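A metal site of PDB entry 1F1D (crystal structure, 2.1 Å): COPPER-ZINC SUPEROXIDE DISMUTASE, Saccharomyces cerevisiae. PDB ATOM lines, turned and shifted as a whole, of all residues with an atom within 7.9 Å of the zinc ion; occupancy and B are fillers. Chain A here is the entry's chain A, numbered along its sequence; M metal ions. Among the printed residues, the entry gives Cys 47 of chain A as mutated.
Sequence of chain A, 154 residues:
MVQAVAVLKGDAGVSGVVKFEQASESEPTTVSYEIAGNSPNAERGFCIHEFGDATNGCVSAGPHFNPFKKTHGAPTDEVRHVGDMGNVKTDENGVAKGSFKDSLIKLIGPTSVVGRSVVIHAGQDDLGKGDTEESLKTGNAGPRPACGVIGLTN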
ATOM      1  N   PHE A  46      35.677  13.441  -3.953  1.00  0.00           N
ATOM      2  CA  PHE A  46      36.145  12.930  -2.667  1.00  0.00           C
ATOM      3  C   PHE A  46      34.922  12.344  -1.948  1.00  0.00           C
ATOM      4  O   PHE A  46      33.947  13.043  -1.714  1.00  0.00           O
ATOM      5  CB  PHE A  46      36.719  14.113  -1.880  1.00  0.00           C
ATOM      6  CG  PHE A  46      37.542  13.724  -0.676  1.00  0.00           C
ATOM      7  CD1 PHE A  46      38.364  12.577  -0.703  1.00  0.00           C
ATOM      8  CD2 PHE A  46      37.548  14.522   0.461  1.00  0.00           C
ATOM      9  CE1 PHE A  46      39.181  12.254   0.395  1.00  0.00           C
ATOM     10  CE2 PHE A  46      38.365  14.206   1.567  1.00  0.00           C
ATOM     11  CZ  PHE A  46      39.183  13.065   1.533  1.00  0.00           C
ATOM     12  N   CYS A  47      34.983  11.060  -1.593  1.00  0.00           N
ATOM     13  CA  CYS A  47      33.852  10.431  -0.906  1.00  0.00           C
ATOM     14  C   CYS A  47      34.080   9.182  -0.049  1.00  0.00           C
ATOM     15  O   CYS A  47      35.057   8.463  -0.208  1.00  0.00           O
ATOM     16  CB  CYS A  47      32.650  10.195  -1.859  1.00  0.00           C
ATOM     17  SG  CYS A  47      32.847  10.128  -3.677  1.00  0.00           S
ATOM     18  N   ILE A  48      33.134   8.949   0.857  1.00  0.00           N
ATOM     19  CA  ILE A  48      33.115   7.784   1.758  1.00  0.00           C
ATOM     20  C   ILE A  48      32.214   6.700   1.170  1.00  0.00           C
ATOM     21  O   ILE A  48      31.047   6.930   0.867  1.00  0.00           O
ATOM     22  CB  ILE A  48      32.610   8.151   3.173  1.00  0.00           C
ATOM     23  CG1 ILE A  48      33.591   9.152   3.810  1.00  0.00           C
ATOM     24  CG2 ILE A  48      32.480   6.881   4.043  1.00  0.00           C
ATOM     25  CD1 ILE A  48      33.129   9.819   5.071  1.00  0.00           C
ATOM     26  N   HIS A  49      32.788   5.539   0.918  1.00  0.00           N
ATOM     27  CA  HIS A  49      32.018   4.440   0.367  1.00  0.00           C
ATOM     28  C   HIS A  49      31.595   3.527   1.489  1.00  0.00           C
ATOM     29  O   HIS A  49      32.242   3.489   2.542  1.00  0.00           O
ATOM     30  CB  HIS A  49      32.797   3.708  -0.707  1.00  0.00           C
ATOM     31  CG  HIS A  49      32.886   4.478  -1.981  1.00  0.00           C
ATOM     32  ND1 HIS A  49      32.419   3.982  -3.178  1.00  0.00           N
ATOM     33  CD2 HIS A  49      33.315   5.742  -2.244  1.00  0.00           C
ATOM     34  CE1 HIS A  49      32.543   4.892  -4.116  1.00  0.00           C
ATOM     35  NE2 HIS A  49      33.089   5.975  -3.579  1.00  0.00           N
ATOM     36  N   PRO A  63      29.246   1.123  -3.049  1.00  0.00           N
ATOM     37  CA  PRO A  63      28.668   2.379  -3.462  1.00  0.00           C
ATOM     38  C   PRO A  63      28.854   3.428  -2.370  1.00  0.00           C
ATOM     39  O   PRO A  63      29.433   3.154  -1.321  1.00  0.00           O
ATOM     40  CB  PRO A  63      27.204   2.003  -3.635  1.00  0.00           C
ATOM     41  CG  PRO A  63      26.984   1.091  -2.481  1.00  0.00           C
ATOM     42  CD  PRO A  63      28.203   0.219  -2.491  1.00  0.00           C
ATOM     43  N   HIS A  64      28.364   4.639  -2.618  1.00  0.00           N
ATOM     44  CA  HIS A  64      28.471   5.701  -1.633  1.00  0.00           C
ATOM     45  C   HIS A  64      27.731   5.338  -0.331  1.00  0.00           C
ATOM     46  O   HIS A  64      26.663   4.672  -0.367  1.00  0.00           O
ATOM     47  CB  HIS A  64      27.890   6.997  -2.197  1.00  0.00           C
ATOM     48  CG  HIS A  64      28.666   7.561  -3.347  1.00  0.00           C
ATOM     49  ND1 HIS A  64      28.326   8.735  -3.972  1.00  0.00           N
ATOM     50  CD2 HIS A  64      29.798   7.122  -3.942  1.00  0.00           C
ATOM     51  CE1 HIS A  64      29.228   9.008  -4.901  1.00  0.00           C
ATOM     52  NE2 HIS A  64      30.132   8.047  -4.904  1.00  0.00           N
ATOM     53  N   PHE A  65      28.310   5.709   0.815  1.00  0.00           N
ATOM     54  CA  PHE A  65      27.674   5.439   2.091  1.00  0.00           C
ATOM     55  C   PHE A  65      26.388   6.319   2.109  1.00  0.00           C
ATOM     56  O   PHE A  65      26.439   7.550   2.122  1.00  0.00           O
ATOM     57  CB  PHE A  65      28.614   5.733   3.265  1.00  0.00           C
ATOM     58  CG  PHE A  65      28.027   5.385   4.601  1.00  0.00           C
ATOM     59  CD1 PHE A  65      27.391   4.152   4.788  1.00  0.00           C
ATOM     60  CD2 PHE A  65      28.038   6.301   5.649  1.00  0.00           C
ATOM     61  CE1 PHE A  65      26.765   3.861   5.986  1.00  0.00           C
ATOM     62  CE2 PHE A  65      27.418   6.011   6.860  1.00  0.00           C
ATOM     63  CZ  PHE A  65      26.772   4.785   7.028  1.00  0.00           C
ATOM     64  N   ASN A  66      25.236   5.661   2.126  1.00  0.00           N
ATOM     65  CA  ASN A  66      23.966   6.368   2.032  1.00  0.00           C
ATOM     66  C   ASN A  66      22.864   5.678   2.861  1.00  0.00           C
ATOM     67  O   ASN A  66      21.887   5.161   2.311  1.00  0.00           O
ATOM     68  CB  ASN A  66      23.649   6.395   0.512  1.00  0.00           C
ATOM     69  CG  ASN A  66      22.300   6.920   0.167  1.00  0.00           C
ATOM     70  OD1 ASN A  66      21.842   7.902   0.714  1.00  0.00           O
ATOM     71  ND2 ASN A  66      21.698   6.322  -0.827  1.00  0.00           N
ATOM     72  N   LYS A  70      19.195   8.588  -0.043  1.00  0.00           N
ATOM     73  CA  LYS A  70      18.906   9.788  -0.808  1.00  0.00           C
ATOM     74  C   LYS A  70      19.749   9.737  -2.088  1.00  0.00           C
ATOM     75  O   LYS A  70      20.485   8.772  -2.331  1.00  0.00           O
ATOM     76  CB  LYS A  70      19.271  11.063  -0.016  1.00  0.00           C
ATOM     77  CG  LYS A  70      18.639  11.178   1.373  1.00  0.00           C
ATOM     78  CD  LYS A  70      17.164  11.523   1.336  1.00  0.00           C
ATOM     79  CE  LYS A  70      16.609  11.852   2.764  1.00  0.00           C
ATOM     80  NZ  LYS A  70      16.020  10.673   3.596  1.00  0.00           N
ATOM     81  N   THR A  71      19.595  10.734  -2.942  1.00  0.00           N
ATOM     82  CA  THR A  71      20.371  10.783  -4.163  1.00  0.00           C
ATOM     83  C   THR A  71      21.651  11.544  -3.839  1.00  0.00           C
ATOM     84  O   THR A  71      21.732  12.273  -2.862  1.00  0.00           O
ATOM     85  CB  THR A  71      19.666  11.553  -5.311  1.00  0.00           C
ATOM     86  OG1 THR A  71      19.293  12.842  -4.859  1.00  0.00           O
ATOM     87  CG2 THR A  71      18.449  10.826  -5.826  1.00  0.00           C
ATOM     88  N   HIS A  72      22.642  11.312  -4.684  1.00  0.00           N
ATOM     89  CA  HIS A  72      23.952  11.937  -4.607  1.00  0.00           C
ATOM     90  C   HIS A  72      23.837  13.445  -4.815  1.00  0.00           C
ATOM     91  O   HIS A  72      23.115  13.900  -5.697  1.00  0.00           O
ATOM     92  CB  HIS A  72      24.828  11.332  -5.698  1.00  0.00           C
ATOM     93  CG  HIS A  72      26.173  11.953  -5.800  1.00  0.00           C
ATOM     94  ND1 HIS A  72      27.234  11.550  -5.014  1.00  0.00           N
ATOM     95  CD2 HIS A  72      26.639  12.956  -6.580  1.00  0.00           C
ATOM     96  CE1 HIS A  72      28.289  12.282  -5.307  1.00  0.00           C
ATOM     97  NE2 HIS A  72      27.947  13.146  -6.245  1.00  0.00           N
ATOM     98  N   GLY A  73      24.563  14.215  -4.024  1.00  0.00           N
ATOM     99  CA  GLY A  73      24.507  15.655  -4.168  1.00  0.00           C
ATOM    100  C   GLY A  73      25.759  16.270  -3.603  1.00  0.00           C
ATOM    101  O   GLY A  73      26.734  15.581  -3.385  1.00  0.00           O
ATOM    102  N   ALA A  74      25.714  17.577  -3.422  1.00  0.00           N
ATOM    103  CA  ALA A  74      26.823  18.365  -2.877  1.00  0.00           C
ATOM    104  C   ALA A  74      26.795  18.350  -1.337  1.00  0.00           C
ATOM    105  O   ALA A  74      25.718  18.240  -0.726  1.00  0.00           O
ATOM    106  CB  ALA A  74      26.756  19.808  -3.402  1.00  0.00           C
ATOM    107  N   ARG A  80      21.632  14.648  -0.198  1.00  0.00           N
ATOM    108  CA  ARG A  80      22.958  14.193  -0.562  1.00  0.00           C
ATOM    109  C   ARG A  80      23.135  12.858   0.144  1.00  0.00           C
ATOM    110  O   ARG A  80      22.276  12.452   0.949  1.00  0.00           O
ATOM    111  CB  ARG A  80      24.020  15.167  -0.030  1.00  0.00           C
ATOM    112  CG  ARG A  80      23.971  15.385   1.480  1.00  0.00           C
ATOM    113  CD  ARG A  80      25.249  16.020   1.983  1.00  0.00           C
ATOM    114  NE  ARG A  80      26.135  15.041   2.627  1.00  0.00           N
ATOM    115  CZ  ARG A  80      27.046  15.345   3.555  1.00  0.00           C
ATOM    116  NH1 ARG A  80      27.207  16.597   3.934  1.00  0.00           N
ATOM    117  NH2 ARG A  80      27.779  14.400   4.119  1.00  0.00           N
ATOM    118  N   HIS A  81      24.200  12.136  -0.199  1.00  0.00           N
ATOM    119  CA  HIS A  81      24.496  10.891   0.484  1.00  0.00           C
ATOM    120  C   HIS A  81      25.328  11.313   1.693  1.00  0.00           C
ATOM    121  O   HIS A  81      26.030  12.333   1.640  1.00  0.00           O
ATOM    122  CB  HIS A  81      25.325   9.976  -0.413  1.00  0.00           C
ATOM    123  CG  HIS A  81      24.576   9.459  -1.604  1.00  0.00           C
ATOM    124  ND1 HIS A  81      25.201   9.149  -2.802  1.00  0.00           N
ATOM    125  CD2 HIS A  81      23.276   9.147  -1.764  1.00  0.00           C
ATOM    126  CE1 HIS A  81      24.297   8.654  -3.644  1.00  0.00           C
ATOM    127  NE2 HIS A  81      23.133   8.644  -3.028  1.00  0.00           N
ATOM    128  N   VAL A  82      25.244  10.572   2.798  1.00  0.00           N
ATOM    129  CA  VAL A  82      26.056  10.910   3.965  1.00  0.00           C
ATOM    130  C   VAL A  82      27.541  10.978   3.598  1.00  0.00           C
ATOM    131  O   VAL A  82      28.256  11.857   4.073  1.00  0.00           O
ATOM    132  CB  VAL A  82      25.839   9.855   5.063  1.00  0.00           C
ATOM    133  CG1 VAL A  82      26.923   9.914   6.110  1.00  0.00           C
ATOM    134  CG2 VAL A  82      24.485  10.096   5.694  1.00  0.00           C
ATOM    135  N   GLY A  83      27.969  10.072   2.713  1.00  0.00           N
ATOM    136  CA  GLY A  83      29.351  10.002   2.276  1.00  0.00           C
ATOM    137  C   GLY A  83      29.827  11.000   1.221  1.00  0.00           C
ATOM    138  O   GLY A  83      30.968  10.930   0.797  1.00  0.00           O
ATOM    139  N   ASP A  84      28.960  11.936   0.827  1.00  0.00           N
ATOM    140  CA  ASP A  84      29.307  12.929  -0.187  1.00  0.00           C
ATOM    141  C   ASP A  84      30.151  14.063   0.382  1.00  0.00           C
ATOM    142  O   ASP A  84      29.669  14.872   1.155  1.00  0.00           O
ATOM    143  CB  ASP A  84      28.043  13.483  -0.874  1.00  0.00           C
ATOM    144  CG  ASP A  84      27.327  12.433  -1.741  1.00  0.00           C
ATOM    145  OD1 ASP A  84      26.153  12.611  -2.078  1.00  0.00           O
ATOM    146  OD2 ASP A  84      27.913  11.389  -2.122  1.00  0.00           O
ATOM    147  N   MET A  85      31.425  14.105  -0.005  1.00  0.00           N
ATOM    148  CA  MET A  85      32.357  15.144   0.415  1.00  0.00           C
ATOM    149  C   MET A  85      32.755  16.038  -0.758  1.00  0.00           C
ATOM    150  O   MET A  85      33.728  16.775  -0.675  1.00  0.00           O
ATOM    151  CB  MET A  85      33.597  14.532   1.075  1.00  0.00           C
ATOM    152  CG  MET A  85      33.273  13.618   2.221  1.00  0.00           C
ATOM    153  SD  MET A  85      34.704  13.168   3.174  1.00  0.00           S
ATOM    154  CE  MET A  85      35.255  11.750   2.307  1.00  0.00           C
ATOM    155  N   GLY A  86      32.018  15.919  -1.863  1.00  0.00           N
ATOM    156  CA  GLY A  86      32.236  16.758  -3.028  1.00  0.00           C
ATOM    157  C   GLY A  86      33.551  16.660  -3.756  1.00  0.00           C
ATOM    158  O   GLY A  86      34.014  15.563  -4.037  1.00  0.00           O
ATOM    159  N   ASP A 125      33.544  15.452  -9.513  1.00  0.00           N
ATOM    160  CA  ASP A 125      32.186  15.088  -9.130  1.00  0.00           C
ATOM    161  C   ASP A 125      31.259  16.161  -9.710  1.00  0.00           C
ATOM    162  O   ASP A 125      31.486  17.348  -9.481  1.00  0.00           O
ATOM    163  CB  ASP A 125      32.083  15.127  -7.624  1.00  0.00           C
ATOM    164  CG  ASP A 125      30.736  14.659  -7.097  1.00  0.00           C
ATOM    165  OD1 ASP A 125      29.690  14.753  -7.764  1.00  0.00           O
ATOM    166  OD2 ASP A 125      30.762  14.158  -5.966  1.00  0.00           O
ATOM    167  N   GLY A 128      25.919  15.815  -8.551  1.00  0.00           N
ATOM    168  CA  GLY A 128      24.572  15.331  -8.778  1.00  0.00           C
ATOM    169  C   GLY A 128      23.759  16.275  -9.644  1.00  0.00           C
ATOM    170  O   GLY A 128      22.539  16.117  -9.748  1.00  0.00           O
ATOM    171  N   SER A 135      24.428  10.637 -12.453  1.00  0.00           N
ATOM    172  CA  SER A 135      24.675  11.840 -11.682  1.00  0.00           C
ATOM    173  C   SER A 135      24.145  11.694 -10.254  1.00  0.00           C
ATOM    174  O   SER A 135      24.889  11.894  -9.298  1.00  0.00           O
ATOM    175  CB  SER A 135      24.011  13.018 -12.393  1.00  0.00           C
ATOM    176  OG  SER A 135      24.501  14.260 -11.924  1.00  0.00           O
ATOM    177  N   LEU A 136      22.894  11.259 -10.156  1.00  0.00           N
ATOM    178  CA  LEU A 136      22.192  11.073  -8.889  1.00  0.00           C
ATOM    179  C   LEU A 136      22.674   9.842  -8.117  1.00  0.00           C
ATOM    180  O   LEU A 136      22.381   9.646  -6.933  1.00  0.00           O
ATOM    181  CB  LEU A 136      20.696  10.984  -9.158  1.00  0.00           C
ATOM    182  CG  LEU A 136      20.048  12.265  -9.705  1.00  0.00           C
ATOM    183  CD1 LEU A 136      18.595  12.004 -10.074  1.00  0.00           C
ATOM    184  CD2 LEU A 136      20.140  13.371  -8.663  1.00  0.00           C
ATOM    185  N   LYS A 137      23.394   8.990  -8.833  1.00  0.00           N
ATOM    186  CA  LYS A 137      23.937   7.778  -8.266  1.00  0.00           C
ATOM    187  C   LYS A 137      25.329   8.075  -7.732  1.00  0.00           C
ATOM    188  O   LYS A 137      25.590   7.982  -6.536  1.00  0.00           O
ATOM    189  CB  LYS A 137      24.078   6.703  -9.349  1.00  0.00           C
ATOM    190  CG  LYS A 137      22.840   5.873  -9.565  1.00  0.00           C
ATOM    191  CD  LYS A 137      22.918   4.575  -8.764  1.00  0.00           C
ATOM    192  CE  LYS A 137      21.552   3.861  -8.681  1.00  0.00           C
ATOM    193  NZ  LYS A 137      20.528   4.636  -7.889  1.00  0.00           N
ATOM    194  N   THR A 138      26.181   8.524  -8.634  1.00  0.00           N
ATOM    195  CA  THR A 138      27.574   8.741  -8.316  1.00  0.00           C
ATOM    196  C   THR A 138      28.161  10.126  -8.469  1.00  0.00           C
ATOM    197  O   THR A 138      29.081  10.479  -7.741  1.00  0.00           O
ATOM    198  CB  THR A 138      28.422   7.783  -9.174  1.00  0.00           C
ATOM    199  OG1 THR A 138      28.379   8.208 -10.537  1.00  0.00           O
ATOM    200  CG2 THR A 138      27.869   6.375  -9.071  1.00  0.00           C
ATOM    201  N   GLY A 139      27.661  10.934  -9.399  1.00  0.00           N
ATOM    202  CA  GLY A 139      28.249  12.250  -9.610  1.00  0.00           C
ATOM    203  C   GLY A 139      29.243  12.184 -10.771  1.00  0.00           C
ATOM    204  O   GLY A 139      29.942  13.154 -11.055  1.00  0.00           O
HETATM  205 ZN    ZN M   1      27.202  10.265  -3.366  1.00  0.00          ZN
HETATM  206 CU    CU M   2      33.313   7.698  -4.952  1.00  0.00          CU
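The nearest printed residue that does not touch the zinc ion is Lys 137 (4.2 Å).
O of Lys 70 sits at hydrogen-bond distance from NE2 of His 81, at 2.7 Å.
The side-chain sulfur (SG) of Cys 47 lies close to a ring nitrogen (NE2) of His 64.
The backbone carbonyl oxygen (O) of Leu 136 sits at hydrogen-bond distance from the backbone NH (N) of His 72 (2.8 Å).
The side-chain carboxylate (OD1) of Asp 84 sits at hydrogen-bond distance from the backbone NH (N) of Gly 73, at 3.0 Å.
NE2 of His 72 sits at hydrogen-bond distance from OD1 of Asp 125 (2.8 Å).
NE2 of His 72 lies close to O of Thr 138, 3.3 Å away.
The zinc ion is bound by OD2 of Asp 84, ND1 of His 64, ND1 of His 72 and ND1 of His 81.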
